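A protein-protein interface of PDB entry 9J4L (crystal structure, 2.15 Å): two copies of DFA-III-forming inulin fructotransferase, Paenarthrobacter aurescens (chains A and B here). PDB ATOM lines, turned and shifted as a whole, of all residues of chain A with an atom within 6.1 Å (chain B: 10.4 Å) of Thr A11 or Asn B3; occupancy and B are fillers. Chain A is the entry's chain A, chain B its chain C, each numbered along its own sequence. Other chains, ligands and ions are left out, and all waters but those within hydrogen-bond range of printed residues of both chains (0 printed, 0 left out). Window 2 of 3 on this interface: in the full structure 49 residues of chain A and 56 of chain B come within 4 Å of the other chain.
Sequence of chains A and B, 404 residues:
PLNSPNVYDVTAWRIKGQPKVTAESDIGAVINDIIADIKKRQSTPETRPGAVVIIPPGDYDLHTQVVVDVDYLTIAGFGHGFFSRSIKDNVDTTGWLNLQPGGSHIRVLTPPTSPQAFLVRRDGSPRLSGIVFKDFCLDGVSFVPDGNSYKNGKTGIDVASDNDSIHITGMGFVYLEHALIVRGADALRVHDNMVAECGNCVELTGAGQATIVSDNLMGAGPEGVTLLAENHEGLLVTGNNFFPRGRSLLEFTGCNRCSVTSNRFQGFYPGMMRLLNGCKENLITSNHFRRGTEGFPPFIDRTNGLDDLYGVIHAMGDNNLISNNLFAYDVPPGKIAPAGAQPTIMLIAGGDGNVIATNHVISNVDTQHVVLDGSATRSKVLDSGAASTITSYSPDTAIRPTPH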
ATOM      1  N   ASP A   9      -5.839  -2.382  23.055  1.00  0.00           N
ATOM      2  CA  ASP A   9      -6.329  -3.610  22.416  1.00  0.00           C
ATOM      3  C   ASP A   9      -5.934  -4.812  23.311  1.00  0.00           C
ATOM      4  O   ASP A   9      -4.739  -4.990  23.568  1.00  0.00           O
ATOM      5  CB  ASP A   9      -5.661  -3.660  21.035  1.00  0.00           C
ATOM      6  CG  ASP A   9      -5.825  -4.986  20.325  1.00  0.00           C
ATOM      7  OD1 ASP A   9      -6.567  -5.860  20.812  1.00  0.00           O
ATOM      8  OD2 ASP A   9      -5.225  -5.129  19.229  1.00  0.00           O
ATOM      9  N   VAL A  10      -6.909  -5.538  23.892  1.00  0.00           N
ATOM     10  CA  VAL A  10      -6.569  -6.654  24.817  1.00  0.00           C
ATOM     11  C   VAL A  10      -5.721  -7.719  24.152  1.00  0.00           C
ATOM     12  O   VAL A  10      -5.053  -8.487  24.831  1.00  0.00           O
ATOM     13  CB  VAL A  10      -7.777  -7.400  25.474  1.00  0.00           C
ATOM     14  CG1 VAL A  10      -8.475  -6.578  26.548  1.00  0.00           C
ATOM     15  CG2 VAL A  10      -8.739  -7.996  24.456  1.00  0.00           C
ATOM     16  N   THR A  11      -5.827  -7.835  22.831  1.00  0.00           N
ATOM     17  CA  THR A  11      -5.038  -8.831  22.104  1.00  0.00           C
ATOM     18  C   THR A  11      -3.596  -8.372  21.874  1.00  0.00           C
ATOM     19  O   THR A  11      -2.712  -9.179  21.607  1.00  0.00           O
ATOM     20  CB  THR A  11      -5.690  -9.235  20.760  1.00  0.00           C
ATOM     21  OG1 THR A  11      -5.859  -8.079  19.932  1.00  0.00           O
ATOM     22  CG2 THR A  11      -7.040  -9.883  20.977  1.00  0.00           C
ATOM     23  N   ALA A  12      -3.340  -7.076  21.994  1.00  0.00           N
ATOM     24  CA  ALA A  12      -1.990  -6.573  21.775  1.00  0.00           C
ATOM     25  C   ALA A  12      -1.208  -6.375  23.087  1.00  0.00           C
ATOM     26  O   ALA A  12       0.006  -6.249  23.080  1.00  0.00           O
ATOM     27  CB  ALA A  12      -2.030  -5.277  20.966  1.00  0.00           C
ATOM     28  N   TRP A  13      -1.890  -6.407  24.217  1.00  0.00           N
ATOM     29  CA  TRP A  13      -1.256  -6.065  25.481  1.00  0.00           C
ATOM     30  C   TRP A  13      -0.454  -7.207  26.029  1.00  0.00           C
ATOM     31  O   TRP A  13      -0.996  -8.269  26.283  1.00  0.00           O
ATOM     32  CB  TRP A  13      -2.306  -5.652  26.491  1.00  0.00           C
ATOM     33  CG  TRP A  13      -1.699  -5.101  27.759  1.00  0.00           C
ATOM     34  CD1 TRP A  13      -1.511  -5.771  28.961  1.00  0.00           C
ATOM     35  CD2 TRP A  13      -1.046  -3.791  27.945  1.00  0.00           C
ATOM     36  NE1 TRP A  13      -0.935  -4.943  29.891  1.00  0.00           N
ATOM     37  CE2 TRP A  13      -0.586  -3.759  29.334  1.00  0.00           C
ATOM     38  CE3 TRP A  13      -0.844  -2.668  27.139  1.00  0.00           C
ATOM     39  CZ2 TRP A  13       0.041  -2.639  29.881  1.00  0.00           C
ATOM     40  CZ3 TRP A  13      -0.190  -1.560  27.697  1.00  0.00           C
ATOM     41  CH2 TRP A  13       0.250  -1.553  29.032  1.00  0.00           C
ATOM     42  N   ALA A  23      -4.972 -12.477  26.533  1.00  0.00           N
ATOM     43  CA  ALA A  23      -6.424 -12.291  26.474  1.00  0.00           C
ATOM     44  C   ALA A  23      -7.160 -13.632  26.412  1.00  0.00           C
ATOM     45  O   ALA A  23      -8.103 -13.849  27.164  1.00  0.00           O
ATOM     46  CB  ALA A  23      -6.804 -11.400  25.305  1.00  0.00           C
ATOM     47  N   GLU A  24      -6.629 -14.576  25.632  1.00  0.00           N
ATOM     48  CA  GLU A  24      -7.187 -15.929  25.559  1.00  0.00           C
ATOM     49  C   GLU A  24      -7.073 -16.697  26.870  1.00  0.00           C
ATOM     50  O   GLU A  24      -8.078 -17.191  27.367  1.00  0.00           O
ATOM     51  CB  GLU A  24      -6.568 -16.748  24.420  1.00  0.00           C
ATOM     52  CG  GLU A  24      -7.149 -16.449  23.059  1.00  0.00           C
ATOM     53  CD  GLU A  24      -6.427 -15.308  22.396  1.00  0.00           C
ATOM     54  OE1 GLU A  24      -5.517 -14.721  23.039  1.00  0.00           O
ATOM     55  OE2 GLU A  24      -6.747 -15.025  21.223  1.00  0.00           O
ATOM     56  N   VAL A  30      -5.161  -9.791  32.159  1.00  0.00           N
ATOM     57  CA  VAL A  30      -4.776  -8.788  31.153  1.00  0.00           C
ATOM     58  C   VAL A  30      -5.397  -7.423  31.457  1.00  0.00           C
ATOM     59  O   VAL A  30      -4.710  -6.419  31.396  1.00  0.00           O
ATOM     60  CB  VAL A  30      -5.111  -9.236  29.701  1.00  0.00           C
ATOM     61  CG1 VAL A  30      -4.740  -8.149  28.687  1.00  0.00           C
ATOM     62  CG2 VAL A  30      -4.412 -10.553  29.374  1.00  0.00           C
ATOM     63  N   ILE A  54     -10.379  -2.378  24.326  1.00  0.00           N
ATOM     64  CA  ILE A  54     -11.024  -2.890  23.133  1.00  0.00           C
ATOM     65  C   ILE A  54     -10.861  -4.411  23.066  1.00  0.00           C
ATOM     66  O   ILE A  54      -9.745  -4.943  23.166  1.00  0.00           O
ATOM     67  CB  ILE A  54     -10.421  -2.282  21.853  1.00  0.00           C
ATOM     68  CG1 ILE A  54     -10.491  -0.757  21.879  1.00  0.00           C
ATOM     69  CG2 ILE A  54     -11.136  -2.832  20.623  1.00  0.00           C
ATOM     70  CD1 ILE A  54     -11.903  -0.224  21.967  1.00  0.00           C
ATOM     71  N   PRO A  56     -11.528  -7.392  20.559  1.00  0.00           N
ATOM     72  CA  PRO A  56     -11.903  -7.921  19.239  1.00  0.00           C
ATOM     73  C   PRO A  56     -12.749  -9.178  19.388  1.00  0.00           C
ATOM     74  O   PRO A  56     -12.666  -9.846  20.405  1.00  0.00           O
ATOM     75  CB  PRO A  56     -10.553  -8.291  18.601  1.00  0.00           C
ATOM     76  CG  PRO A  56      -9.516  -7.582  19.401  1.00  0.00           C
ATOM     77  CD  PRO A  56     -10.074  -7.419  20.785  1.00  0.00           C
ATOM     78  N   TYR A  60     -12.324 -15.837  24.883  1.00  0.00           N
ATOM     79  CA  TYR A  60     -11.340 -15.440  25.875  1.00  0.00           C
ATOM     80  C   TYR A  60     -11.786 -16.021  27.213  1.00  0.00           C
ATOM     81  O   TYR A  60     -12.950 -15.946  27.569  1.00  0.00           O
ATOM     82  CB  TYR A  60     -11.211 -13.896  25.975  1.00  0.00           C
ATOM     83  CG  TYR A  60     -11.044 -13.173  24.654  1.00  0.00           C
ATOM     84  CD1 TYR A  60      -9.798 -13.075  24.044  1.00  0.00           C
ATOM     85  CD2 TYR A  60     -12.129 -12.562  24.025  1.00  0.00           C
ATOM     86  CE1 TYR A  60      -9.636 -12.440  22.819  1.00  0.00           C
ATOM     87  CE2 TYR A  60     -11.981 -11.897  22.807  1.00  0.00           C
ATOM     88  CZ  TYR A  60     -10.726 -11.840  22.216  1.00  0.00           C
ATOM     89  OH  TYR A  60     -10.565 -11.203  21.011  1.00  0.00           O
ATOM     90  N   PRO B   1      -4.916  -4.020  11.921  1.00  0.00           N
ATOM     91  CA  PRO B   1      -5.506  -2.868  12.608  1.00  0.00           C
ATOM     92  C   PRO B   1      -5.546  -3.147  14.101  1.00  0.00           C
ATOM     93  O   PRO B   1      -4.918  -2.456  14.888  1.00  0.00           O
ATOM     94  CB  PRO B   1      -6.941  -2.807  12.055  1.00  0.00           C
ATOM     95  CG  PRO B   1      -7.241  -4.180  11.547  1.00  0.00           C
ATOM     96  CD  PRO B   1      -5.929  -4.878  11.265  1.00  0.00           C
ATOM     97  N   LEU B   2      -6.173  -4.244  14.473  1.00  0.00           N
ATOM     98  CA  LEU B   2      -6.031  -4.725  15.832  1.00  0.00           C
ATOM     99  C   LEU B   2      -5.231  -6.031  15.806  1.00  0.00           C
ATOM    100  O   LEU B   2      -4.946  -6.554  14.741  1.00  0.00           O
ATOM    101  CB  LEU B   2      -7.415  -4.880  16.470  1.00  0.00           C
ATOM    102  CG  LEU B   2      -8.064  -3.527  16.814  1.00  0.00           C
ATOM    103  CD1 LEU B   2      -9.581  -3.594  16.852  1.00  0.00           C
ATOM    104  CD2 LEU B   2      -7.554  -2.948  18.131  1.00  0.00           C
ATOM    105  N   ASN B   3      -4.787  -6.519  16.952  1.00  0.00           N
ATOM    106  CA  ASN B   3      -3.955  -7.723  16.951  1.00  0.00           C
ATOM    107  C   ASN B   3      -4.802  -9.010  16.925  1.00  0.00           C
ATOM    108  O   ASN B   3      -4.530  -9.968  17.647  1.00  0.00           O
ATOM    109  CB  ASN B   3      -2.983  -7.715  18.139  1.00  0.00           C
ATOM    110  CG  ASN B   3      -1.834  -8.700  17.970  1.00  0.00           C
ATOM    111  OD1 ASN B   3      -1.235  -8.807  16.903  1.00  0.00           O
ATOM    112  ND2 ASN B   3      -1.499  -9.397  19.041  1.00  0.00           N
ATOM    113  N   SER B   4      -5.866  -8.998  16.127  1.00  0.00           N
ATOM    114  CA  SER B   4      -6.776 -10.137  16.053  1.00  0.00           C
ATOM    115  C   SER B   4      -7.058 -10.501  14.602  1.00  0.00           C
ATOM    116  O   SER B   4      -7.333  -9.626  13.794  1.00  0.00           O
ATOM    117  CB  SER B   4      -8.083  -9.826  16.771  1.00  0.00           C
ATOM    118  OG  SER B   4      -9.031 -10.854  16.567  1.00  0.00           O
ATOM    119  N   PRO B   5      -7.026 -11.802  14.274  1.00  0.00           N
ATOM    120  CA  PRO B   5      -7.409 -12.186  12.915  1.00  0.00           C
ATOM    121  C   PRO B   5      -8.907 -11.961  12.658  1.00  0.00           C
ATOM    122  O   PRO B   5      -9.347 -12.047  11.517  1.00  0.00           O
ATOM    123  CB  PRO B   5      -7.067 -13.679  12.846  1.00  0.00           C
ATOM    124  CG  PRO B   5      -6.829 -14.133  14.260  1.00  0.00           C
ATOM    125  CD  PRO B   5      -6.865 -12.953  15.183  1.00  0.00           C
ATOM    126  N   ASN B   6      -9.660 -11.642  13.707  1.00  0.00           N
ATOM    127  CA  ASN B   6     -11.125 -11.529  13.617  1.00  0.00           C
ATOM    128  C   ASN B   6     -11.631 -10.108  13.370  1.00  0.00           C
ATOM    129  O   ASN B   6     -12.836  -9.854  13.457  1.00  0.00           O
ATOM    130  CB  ASN B   6     -11.777 -12.121  14.869  1.00  0.00           C
ATOM    131  CG  ASN B   6     -11.414 -13.587  15.059  1.00  0.00           C
ATOM    132  OD1 ASN B   6     -11.159 -14.294  14.088  1.00  0.00           O
ATOM    133  ND2 ASN B   6     -11.435 -14.059  16.308  1.00  0.00           N
ATOM    134  N   VAL B   7     -10.718  -9.188  13.069  1.00  0.00           N
ATOM    135  CA  VAL B   7     -11.072  -7.804  12.770  1.00  0.00           C
ATOM    136  C   VAL B   7     -10.634  -7.479  11.346  1.00  0.00           C
ATOM    137  O   VAL B   7      -9.476  -7.631  11.003  1.00  0.00           O
ATOM    138  CB  VAL B   7     -10.404  -6.831  13.775  1.00  0.00           C
ATOM    139  CG1 VAL B   7     -10.723  -5.375  13.435  1.00  0.00           C
ATOM    140  CG2 VAL B   7     -10.847  -7.168  15.193  1.00  0.00           C
ATOM    141  N   TYR B   8     -11.581  -7.182  10.477  1.00  0.00           N
ATOM    142  CA  TYR B   8     -11.239  -6.911   9.082  1.00  0.00           C
ATOM    143  C   TYR B   8     -11.592  -5.474   8.672  1.00  0.00           C
ATOM    144  O   TYR B   8     -12.728  -5.038   8.831  1.00  0.00           O
ATOM    145  CB  TYR B   8     -11.960  -7.884   8.144  1.00  0.00           C
ATOM    146  CG  TYR B   8     -11.631  -9.354   8.343  1.00  0.00           C
ATOM    147  CD1 TYR B   8     -12.344 -10.123   9.252  1.00  0.00           C
ATOM    148  CD2 TYR B   8     -10.696  -9.995   7.518  1.00  0.00           C
ATOM    149  CE1 TYR B   8     -12.091 -11.480   9.395  1.00  0.00           C
ATOM    150  CE2 TYR B   8     -10.439 -11.353   7.654  1.00  0.00           C
ATOM    151  CZ  TYR B   8     -11.136 -12.084   8.602  1.00  0.00           C
ATOM    152  OH  TYR B   8     -10.887 -13.423   8.747  1.00  0.00           O
ATOM    153  N   ARG B  41     -10.389 -20.270   9.052  1.00  0.00           N
ATOM    154  CA  ARG B  41      -9.845 -20.247  10.409  1.00  0.00           C
ATOM    155  C   ARG B  41     -10.804 -20.782  11.478  1.00  0.00           C
ATOM    156  O   ARG B  41     -10.373 -21.373  12.467  1.00  0.00           O
ATOM    157  CB  ARG B  41      -9.338 -18.848  10.790  1.00  0.00           C
ATOM    158  CG  ARG B  41      -8.369 -18.230   9.787  1.00  0.00           C
ATOM    159  CD  ARG B  41      -8.049 -16.781  10.139  1.00  0.00           C
ATOM    160  NE  ARG B  41      -9.241 -15.916  10.199  1.00  0.00           N
ATOM    161  CZ  ARG B  41      -9.908 -15.639  11.318  1.00  0.00           C
ATOM    162  NH1 ARG B  41      -9.534 -16.206  12.451  1.00  0.00           N
ATOM    163  NH2 ARG B  41     -10.955 -14.818  11.310  1.00  0.00           N
ATOM    164  N   VAL B  52     -15.569  -8.970  13.017  1.00  0.00           N
ATOM    165  CA  VAL B  52     -16.076  -7.689  12.629  1.00  0.00           C
ATOM    166  C   VAL B  52     -15.520  -7.204  11.313  1.00  0.00           C
ATOM    167  O   VAL B  52     -14.336  -7.191  11.094  1.00  0.00           O
ATOM    168  CB  VAL B  52     -15.953  -6.615  13.727  1.00  0.00           C
ATOM    169  CG1 VAL B  52     -14.586  -6.499  14.311  1.00  0.00           C
ATOM    170  CG2 VAL B  52     -16.514  -5.303  13.304  1.00  0.00           C
ATOM    171  N   ILE B  54     -15.126  -4.008   9.070  1.00  0.00           N
ATOM    172  CA  ILE B  54     -15.187  -2.557   9.291  1.00  0.00           C
ATOM    173  C   ILE B  54     -15.272  -1.817   7.965  1.00  0.00           C
ATOM    174  O   ILE B  54     -14.462  -2.041   7.080  1.00  0.00           O
ATOM    175  CB  ILE B  54     -14.003  -2.069  10.158  1.00  0.00           C
ATOM    176  CG1 ILE B  54     -14.157  -2.599  11.586  1.00  0.00           C
ATOM    177  CG2 ILE B  54     -13.895  -0.533  10.205  1.00  0.00           C
ATOM    178  CD1 ILE B  54     -12.889  -2.452  12.393  1.00  0.00           C
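1 position is printed for both chains. Of the 7 pairs that touch across the chains among the printed residues, none has its exchanged pair printed and touching as well.
OD1 of Asp A9 lies within hydrogen-bond range of OG1 of Thr A11 (2.5 Å). OH of Tyr A60 lies within hydrogen-bond range of O of Pro A56, 2.6 Å away. N of Asn B6 sits close to OG of Ser B4 (3.0 Å).
Among the printed residues, merely in contact across the chains: Asp A9 with Leu B2 (3.4 Å), Thr A11 with Ser B4 (3.9 Å), Ala A12 with Asn B3 (3.9 Å), Pro A56 with Ser B4 (3.4 Å) and Pro A56 with Val B7 (3.6 Å).
Of chain B, only Asn B3 and Ser B4 come within 4 Å of Thr A11. Asn B3 touches just these residues of chain A: Asp A9, Thr A11 and Ala A12. No residue of chain B comes within 4 Å of Val A10. Ala A12 touches just one residue of chain B: Asn B3 (3.9 Å). Pro A56 touches two residues of chain B. Of the printed residues of chain A, Leu B2 touches Asp A9. Printed residues of chain A within 4 Å of Ser B4: Thr A11 and Pro A56. Of the printed residues of chain A, Val B7 touches Pro A56 (3.6 Å). Trp A13 touches none of the printed residues of chain B. The nearest residue of chain B that does not touch Thr A11 is Leu B2 (4.6 Å).
OD2 of Asp A9 lies within hydrogen-bond range of N of Asn B3, 2.7 Å away. The side-chain amide nitrogen (ND2) of Asn B3 lies within hydrogen-bond range of the backbone carbonyl oxygen (O) of Thr A11, at 2.8 Å.
Of the 11 printed residues of chain A, 4 touch a printed residue of chain B. Hydrophobic or aromatic side chains of chain A that line the printed part of chain B: Ala A12 and Pro A56.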
